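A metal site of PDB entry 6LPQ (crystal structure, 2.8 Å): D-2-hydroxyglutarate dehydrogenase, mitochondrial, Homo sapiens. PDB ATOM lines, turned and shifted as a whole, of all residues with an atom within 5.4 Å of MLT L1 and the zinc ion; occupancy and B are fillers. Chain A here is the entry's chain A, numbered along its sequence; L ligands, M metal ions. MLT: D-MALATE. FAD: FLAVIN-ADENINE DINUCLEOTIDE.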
ATOM      1  N   MET A  89      -0.813 -29.774   6.154  1.00  0.00           N
ATOM      2  CA  MET A  89      -0.734 -30.834   7.144  1.00  0.00           C
ATOM      3  C   MET A  89      -0.588 -32.226   6.529  1.00  0.00           C
ATOM      4  O   MET A  89      -0.510 -33.212   7.269  1.00  0.00           O
ATOM      5  CB  MET A  89      -1.952 -30.782   8.077  1.00  0.00           C
ATOM      6  CG  MET A  89      -1.937 -29.465   8.796  1.00  0.00           C
ATOM      7  SD  MET A  89      -0.968 -29.456  10.311  1.00  0.00           S
ATOM      8  CE  MET A  89      -2.238 -29.375  11.558  1.00  0.00           C
ATOM      9  N   GLY A 164     -11.925 -23.816   8.415  1.00  0.00           N
ATOM     10  CA  GLY A 164     -11.525 -22.969   9.512  1.00  0.00           C
ATOM     11  C   GLY A 164     -12.652 -22.575  10.448  1.00  0.00           C
ATOM     12  O   GLY A 164     -13.700 -23.217  10.538  1.00  0.00           O
ATOM     13  N   LEU A 165     -12.411 -21.471  11.161  1.00  0.00           N
ATOM     14  CA  LEU A 165     -13.122 -21.135  12.384  1.00  0.00           C
ATOM     15  C   LEU A 165     -14.374 -20.310  12.158  1.00  0.00           C
ATOM     16  O   LEU A 165     -15.174 -20.155  13.094  1.00  0.00           O
ATOM     17  CB  LEU A 165     -12.179 -20.399  13.343  1.00  0.00           C
ATOM     18  CG  LEU A 165     -10.859 -21.114  13.621  1.00  0.00           C
ATOM     19  CD1 LEU A 165      -9.836 -20.154  14.213  1.00  0.00           C
ATOM     20  CD2 LEU A 165     -11.057 -22.318  14.516  1.00  0.00           C
ATOM     21  N   GLU A 265     -17.032 -24.212  18.462  1.00  0.00           N
ATOM     22  CA  GLU A 265     -15.891 -25.100  18.551  1.00  0.00           C
ATOM     23  C   GLU A 265     -15.965 -25.856  19.871  1.00  0.00           C
ATOM     24  O   GLU A 265     -16.553 -25.360  20.846  1.00  0.00           O
ATOM     25  CB  GLU A 265     -14.577 -24.314  18.497  1.00  0.00           C
ATOM     26  CG  GLU A 265     -14.334 -23.559  17.198  1.00  0.00           C
ATOM     27  CD  GLU A 265     -14.073 -24.464  16.031  1.00  0.00           C
ATOM     28  OE1 GLU A 265     -13.307 -25.441  16.199  1.00  0.00           O
ATOM     29  OE2 GLU A 265     -14.617 -24.200  14.943  1.00  0.00           O
ATOM     30  N   ARG A 340      -8.412 -22.373  21.976  1.00  0.00           N
ATOM     31  CA  ARG A 340      -8.786 -23.289  20.912  1.00  0.00           C
ATOM     32  C   ARG A 340      -7.759 -23.289  19.789  1.00  0.00           C
ATOM     33  O   ARG A 340      -7.320 -24.348  19.343  1.00  0.00           O
ATOM     34  CB  ARG A 340     -10.179 -22.921  20.372  1.00  0.00           C
ATOM     35  CG  ARG A 340     -10.541 -23.556  19.037  1.00  0.00           C
ATOM     36  CD  ARG A 340     -10.540 -25.081  19.101  1.00  0.00           C
ATOM     37  NE  ARG A 340     -10.799 -25.642  17.776  1.00  0.00           N
ATOM     38  CZ  ARG A 340      -9.860 -25.847  16.857  1.00  0.00           C
ATOM     39  NH1 ARG A 340      -8.595 -25.582  17.126  1.00  0.00           N
ATOM     40  NH2 ARG A 340     -10.185 -26.348  15.678  1.00  0.00           N
ATOM     41  N   GLU A 341      -7.390 -22.086  19.322  1.00  0.00           N
ATOM     42  CA  GLU A 341      -6.513 -21.961  18.161  1.00  0.00           C
ATOM     43  C   GLU A 341      -5.162 -22.655  18.364  1.00  0.00           C
ATOM     44  O   GLU A 341      -4.587 -23.172  17.402  1.00  0.00           O
ATOM     45  CB  GLU A 341      -6.264 -20.485  17.846  1.00  0.00           C
ATOM     46  CG  GLU A 341      -7.425 -19.769  17.175  1.00  0.00           C
ATOM     47  CD  GLU A 341      -7.109 -18.319  16.880  1.00  0.00           C
ATOM     48  OE1 GLU A 341      -6.275 -17.729  17.606  1.00  0.00           O
ATOM     49  OE2 GLU A 341      -7.689 -17.762  15.931  1.00  0.00           O
ATOM     50  N   THR A 344      -3.456 -27.246  18.283  1.00  0.00           N
ATOM     51  CA  THR A 344      -2.593 -27.861  17.288  1.00  0.00           C
ATOM     52  C   THR A 344      -1.109 -27.699  17.624  1.00  0.00           C
ATOM     53  O   THR A 344      -0.299 -28.597  17.390  1.00  0.00           O
ATOM     54  CB  THR A 344      -2.889 -27.254  15.919  1.00  0.00           C
ATOM     55  OG1 THR A 344      -4.287 -27.386  15.625  1.00  0.00           O
ATOM     56  CG2 THR A 344      -2.066 -27.922  14.827  1.00  0.00           C
ATOM     57  N   LYS A 355      -2.269 -37.673  13.291  1.00  0.00           N
ATOM     58  CA  LYS A 355      -3.258 -36.621  13.038  1.00  0.00           C
ATOM     59  C   LYS A 355      -4.308 -37.106  12.063  1.00  0.00           C
ATOM     60  O   LYS A 355      -3.973 -37.547  10.953  1.00  0.00           O
ATOM     61  CB  LYS A 355      -2.593 -35.356  12.494  1.00  0.00           C
ATOM     62  CG  LYS A 355      -3.557 -34.186  12.374  1.00  0.00           C
ATOM     63  CD  LYS A 355      -2.828 -32.893  12.065  1.00  0.00           C
ATOM     64  CE  LYS A 355      -1.999 -32.425  13.251  1.00  0.00           C
ATOM     65  NZ  LYS A 355      -2.863 -32.114  14.423  1.00  0.00           N
ATOM     66  N   TYR A 386     -11.154 -32.677  19.227  1.00  0.00           N
ATOM     67  CA  TYR A 386     -11.600 -31.293  19.208  1.00  0.00           C
ATOM     68  C   TYR A 386     -12.028 -30.907  17.800  1.00  0.00           C
ATOM     69  O   TYR A 386     -11.918 -31.703  16.862  1.00  0.00           O
ATOM     70  CB  TYR A 386     -10.496 -30.383  19.776  1.00  0.00           C
ATOM     71  CG  TYR A 386      -9.248 -30.317  18.918  1.00  0.00           C
ATOM     72  CD1 TYR A 386      -8.291 -31.327  18.995  1.00  0.00           C
ATOM     73  CD2 TYR A 386      -9.019 -29.271  18.046  1.00  0.00           C
ATOM     74  CE1 TYR A 386      -7.149 -31.284  18.231  1.00  0.00           C
ATOM     75  CE2 TYR A 386      -7.870 -29.216  17.276  1.00  0.00           C
ATOM     76  CZ  TYR A 386      -6.938 -30.228  17.372  1.00  0.00           C
ATOM     77  OH  TYR A 386      -5.796 -30.185  16.608  1.00  0.00           O
ATOM     78  N   GLY A 387     -12.507 -29.671  17.651  1.00  0.00           N
ATOM     79  CA  GLY A 387     -12.649 -29.071  16.341  1.00  0.00           C
ATOM     80  C   GLY A 387     -14.026 -28.511  16.037  1.00  0.00           C
ATOM     81  O   GLY A 387     -14.779 -28.138  16.939  1.00  0.00           O
ATOM     82  N   HIS A 388     -14.351 -28.444  14.743  1.00  0.00           N
ATOM     83  CA  HIS A 388     -15.508 -27.699  14.252  1.00  0.00           C
ATOM     84  C   HIS A 388     -16.747 -28.584  14.332  1.00  0.00           C
ATOM     85  O   HIS A 388     -17.225 -29.133  13.346  1.00  0.00           O
ATOM     86  CB  HIS A 388     -15.247 -27.208  12.829  1.00  0.00           C
ATOM     87  CG  HIS A 388     -13.825 -26.802  12.599  1.00  0.00           C
ATOM     88  ND1 HIS A 388     -13.308 -25.601  13.040  1.00  0.00           N
ATOM     89  CD2 HIS A 388     -12.806 -27.452  11.994  1.00  0.00           C
ATOM     90  CE1 HIS A 388     -12.024 -25.526  12.702  1.00  0.00           C
ATOM     91  NE2 HIS A 388     -11.698 -26.639  12.070  1.00  0.00           N
ATOM     92  N   ASN A 393     -16.941 -31.816  11.939  1.00  0.00           N
ATOM     93  CA  ASN A 393     -15.545 -32.034  11.564  1.00  0.00           C
ATOM     94  C   ASN A 393     -14.802 -32.234  12.877  1.00  0.00           C
ATOM     95  O   ASN A 393     -14.656 -31.302  13.670  1.00  0.00           O
ATOM     96  CB  ASN A 393     -14.983 -30.853  10.775  1.00  0.00           C
ATOM     97  CG  ASN A 393     -13.533 -31.054  10.343  1.00  0.00           C
ATOM     98  OD1 ASN A 393     -12.910 -30.151   9.791  1.00  0.00           O
ATOM     99  ND2 ASN A 393     -13.006 -32.252  10.556  1.00  0.00           N
ATOM    100  N   HIS A 395     -11.296 -33.195  14.780  1.00  0.00           N
ATOM    101  CA  HIS A 395      -9.851 -33.355  14.757  1.00  0.00           C
ATOM    102  C   HIS A 395      -9.484 -34.415  15.791  1.00  0.00           C
ATOM    103  O   HIS A 395      -9.675 -34.200  16.995  1.00  0.00           O
ATOM    104  CB  HIS A 395      -9.148 -32.030  15.027  1.00  0.00           C
ATOM    105  CG  HIS A 395      -9.410 -31.002  13.977  1.00  0.00           C
ATOM    106  ND1 HIS A 395      -9.193 -31.246  12.639  1.00  0.00           N
ATOM    107  CD2 HIS A 395      -9.884 -29.736  14.058  1.00  0.00           C
ATOM    108  CE1 HIS A 395      -9.520 -30.166  11.946  1.00  0.00           C
ATOM    109  NE2 HIS A 395      -9.942 -29.236  12.781  1.00  0.00           N
ATOM    110  N   ASN A 397      -6.496 -36.677  17.300  1.00  0.00           N
ATOM    111  CA  ASN A 397      -5.041 -36.778  17.403  1.00  0.00           C
ATOM    112  C   ASN A 397      -4.666 -37.750  18.517  1.00  0.00           C
ATOM    113  O   ASN A 397      -5.311 -37.785  19.573  1.00  0.00           O
ATOM    114  CB  ASN A 397      -4.427 -35.405  17.654  1.00  0.00           C
ATOM    115  CG  ASN A 397      -4.534 -34.497  16.438  1.00  0.00           C
ATOM    116  OD1 ASN A 397      -3.613 -34.397  15.636  1.00  0.00           O
ATOM    117  ND2 ASN A 397      -5.678 -33.825  16.303  1.00  0.00           N
ATOM    118  N   GLU A 429     -10.921 -31.266   5.734  1.00  0.00           N
ATOM    119  CA  GLU A 429     -10.462 -29.910   5.476  1.00  0.00           C
ATOM    120  C   GLU A 429      -9.048 -29.913   4.911  1.00  0.00           C
ATOM    121  O   GLU A 429      -8.787 -29.277   3.879  1.00  0.00           O
ATOM    122  CB  GLU A 429     -10.666 -29.043   6.728  1.00  0.00           C
ATOM    123  CG  GLU A 429      -9.582 -28.954   7.756  1.00  0.00           C
ATOM    124  CD  GLU A 429     -10.040 -28.148   8.955  1.00  0.00           C
ATOM    125  OE1 GLU A 429      -9.392 -28.217  10.009  1.00  0.00           O
ATOM    126  OE2 GLU A 429     -11.088 -27.473   8.840  1.00  0.00           O
ATOM    127  N   HIS A 430      -8.111 -30.608   5.574  1.00  0.00           N
ATOM    128  CA  HIS A 430      -6.688 -30.442   5.323  1.00  0.00           C
ATOM    129  C   HIS A 430      -6.304 -30.937   3.932  1.00  0.00           C
ATOM    130  O   HIS A 430      -5.274 -30.513   3.403  1.00  0.00           O
ATOM    131  CB  HIS A 430      -5.873 -31.217   6.358  1.00  0.00           C
ATOM    132  CG  HIS A 430      -6.075 -30.752   7.763  1.00  0.00           C
ATOM    133  ND1 HIS A 430      -6.019 -31.615   8.850  1.00  0.00           N
ATOM    134  CD2 HIS A 430      -6.313 -29.521   8.277  1.00  0.00           C
ATOM    135  CE1 HIS A 430      -6.229 -30.936   9.960  1.00  0.00           C
ATOM    136  NE2 HIS A 430      -6.407 -29.665   9.647  1.00  0.00           N
HETATM  137  C1  MLT L   1      -7.668 -26.936  13.650  1.00  0.00           C
HETATM  138  O1  MLT L   1      -7.116 -26.839  14.760  1.00  0.00           O
HETATM  139  O2  MLT L   1      -8.918 -26.740  13.594  1.00  0.00           O
HETATM  140  C2  MLT L   1      -6.851 -27.268  12.380  1.00  0.00           C
HETATM  141  O3  MLT L   1      -7.578 -28.072  11.465  1.00  0.00           O
HETATM  142  C3  MLT L   1      -5.537 -27.898  12.813  1.00  0.00           C
HETATM  143  C4  MLT L   1      -5.527 -29.313  13.407  1.00  0.00           C
HETATM  144  O4  MLT L   1      -4.448 -29.893  13.730  1.00  0.00           O
HETATM  145  O5  MLT L   1      -6.639 -29.883  13.573  1.00  0.00           O
HETATM  146  PA  FAD L   2       1.043 -24.609   1.660  1.00  0.00           P
HETATM  147  O1A FAD L   2       2.294 -23.909   1.303  1.00  0.00           O
HETATM  148  O2A FAD L   2       1.118 -25.464   2.935  1.00  0.00           O
HETATM  149  O5B FAD L   2       0.493 -25.482   0.453  1.00  0.00           O
HETATM  150  C5B FAD L   2      -0.508 -26.503   0.670  1.00  0.00           C
HETATM  151  C4B FAD L   2      -0.814 -27.228  -0.626  1.00  0.00           C
HETATM  152  O4B FAD L   2      -1.377 -26.315  -1.586  1.00  0.00           O
HETATM  153  C3B FAD L   2       0.376 -27.890  -1.323  1.00  0.00           C
HETATM  154  O3B FAD L   2      -0.052 -29.049  -2.027  1.00  0.00           O
HETATM  155  C2B FAD L   2       0.842 -26.788  -2.277  1.00  0.00           C
HETATM  156  O2B FAD L   2       1.500 -27.338  -3.420  1.00  0.00           O
HETATM  157  C1B FAD L   2      -0.484 -26.125  -2.665  1.00  0.00           C
HETATM  158  N9A FAD L   2      -0.394 -24.689  -2.938  1.00  0.00           N
HETATM  159  C8A FAD L   2      -0.022 -23.712  -2.052  1.00  0.00           C
HETATM  160  N7A FAD L   2      -0.041 -22.505  -2.558  1.00  0.00           N
HETATM  161  C5A FAD L   2      -0.473 -22.705  -3.868  1.00  0.00           C
HETATM  162  C6A FAD L   2      -0.711 -21.817  -4.934  1.00  0.00           C
HETATM  163  N6A FAD L   2      -0.537 -20.488  -4.853  1.00  0.00           N
HETATM  164  N1A FAD L   2      -1.128 -22.336  -6.107  1.00  0.00           N
HETATM  165  C2A FAD L   2      -1.297 -23.665  -6.195  1.00  0.00           C
HETATM  166  N3A FAD L   2      -1.103 -24.600  -5.254  1.00  0.00           N
HETATM  167  C4A FAD L   2      -0.689 -24.046  -4.103  1.00  0.00           C
HETATM  168  N1  FAD L   2      -6.744 -26.005   7.564  1.00  0.00           N
HETATM  169  C2  FAD L   2      -8.094 -25.895   7.561  1.00  0.00           C
HETATM  170  O2  FAD L   2      -8.782 -26.235   6.592  1.00  0.00           O
HETATM  171  N3  FAD L   2      -8.742 -25.392   8.680  1.00  0.00           N
HETATM  172  C4  FAD L   2      -8.135 -24.970   9.838  1.00  0.00           C
HETATM  173  O4  FAD L   2      -8.816 -24.535  10.775  1.00  0.00           O
HETATM  174  C4X FAD L   2      -6.695 -25.070   9.820  1.00  0.00           C
HETATM  175  N5  FAD L   2      -6.034 -24.683  10.875  1.00  0.00           N
HETATM  176  C5X FAD L   2      -4.656 -24.793  10.873  1.00  0.00           C
HETATM  177  C6  FAD L   2      -3.948 -24.378  11.991  1.00  0.00           C
HETATM  178  C7  FAD L   2      -2.562 -24.466  12.035  1.00  0.00           C
HETATM  179  C7M FAD L   2      -1.831 -24.013  13.273  1.00  0.00           C
HETATM  180  C8  FAD L   2      -1.861 -24.974  10.929  1.00  0.00           C
HETATM  181  C8M FAD L   2      -0.366 -25.070  10.938  1.00  0.00           C
HETATM  182  C9  FAD L   2      -2.571 -25.376   9.799  1.00  0.00           C
HETATM  183  C9A FAD L   2      -3.949 -25.289   9.760  1.00  0.00           C
HETATM  184  N10 FAD L   2      -4.696 -25.690   8.630  1.00  0.00           N
HETATM  185  C10 FAD L   2      -6.080 -25.601   8.636  1.00  0.00           C
HETATM  186  C1' FAD L   2      -4.010 -26.244   7.445  1.00  0.00           C
HETATM  187  C2' FAD L   2      -4.288 -25.470   6.161  1.00  0.00           C
HETATM  188  O2' FAD L   2      -4.503 -26.366   5.066  1.00  0.00           O
HETATM  189  C3' FAD L   2      -3.100 -24.560   5.839  1.00  0.00           C
HETATM  190  O3' FAD L   2      -2.737 -23.846   7.014  1.00  0.00           O
HETATM  191  C4' FAD L   2      -3.419 -23.588   4.716  1.00  0.00           C
HETATM  192  O4' FAD L   2      -4.772 -23.754   4.312  1.00  0.00           O
HETATM  193  C5' FAD L   2      -2.501 -23.754   3.516  1.00  0.00           C
HETATM  194  O5' FAD L   2      -1.793 -22.516   3.295  1.00  0.00           O
HETATM  195  P   FAD L   2      -0.249 -22.502   3.009  1.00  0.00           P
HETATM  196  O1P FAD L   2       0.131 -21.139   2.439  1.00  0.00           O
HETATM  197  O2P FAD L   2       0.497 -22.976   4.199  1.00  0.00           O
HETATM  198  O3P FAD L   2      -0.140 -23.564   1.848  1.00  0.00           O
HETATM  199 ZN    ZN M   1      -9.602 -27.103  11.650  1.00  0.00          ZN
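The guanidinium group (NH1) of Arg 340 lies within salt-bridge range of an oxygen (O1) of MLT L1 (3.1 Å).
NE2 of His 430 sits close to O3 of MLT L1.
O4 of MLT L1 lies within salt-bridge range of NZ of Lys 355 (2.8 Å).
An oxygen (O1) of MLT L1 lies within hydrogen-bond range of the side-chain hydroxyl (OG1) of Thr 344.
OH of Tyr 386 lies within hydrogen-bond range of O5 of MLT L1 (3.2 Å).
The side-chain carboxylate (OE2) of Glu 429 lies close to a nitrogen (N3) of FAD L2, 3.1 Å away.
OE1 of Glu 429 lies close to NE2 of His 430 (3.3 Å).
OE2 of Glu 429 sits close to OD1 of Asn 393.
N of Asn 393 is in hydrogen-bond range of O of His 388 (3.0 Å).
A ring nitrogen (ND1) of His 388 sits at hydrogen-bond distance from the side-chain carboxylate (OE2) of Glu 265.
The backbone carbonyl oxygen of Tyr 386 is in hydrogen-bond range of the backbone NH of His 395 (2.6 Å).
NE of Arg 340 is in salt-bridge range of OE1 of Glu 265 (3.0 Å).
The side-chain amide oxygen (OD1) of Asn 397 lies within hydrogen-bond range of the side-chain amino group (NZ) of Lys 355, at 2.7 Å.
The side-chain hydroxyl (OH) of Tyr 386 is in hydrogen-bond range of the side-chain hydroxyl (OG1) of Thr 344, at 3.3 Å.
Residues that only touch MLT L1: Met 89.
Hydrophobic or aromatic side chains that line MLT L1: Met 89, Tyr 386, His 388, His 395 and His 430.
The nearest printed residue that does not touch MLT L1 is Asn 397 (4.9 Å).
The zinc ion is bound by OE1 of Glu 429 (2.0 Å), O2 of MLT L1 (2.1 Å), NE2 of His 388 (2.2 Å), O3 of MLT L1 (2.3 Å) and NE2 of His 395 (2.4 Å).
Slightly farther from the zinc ion lies O4 of FAD L2 (2.8 Å).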
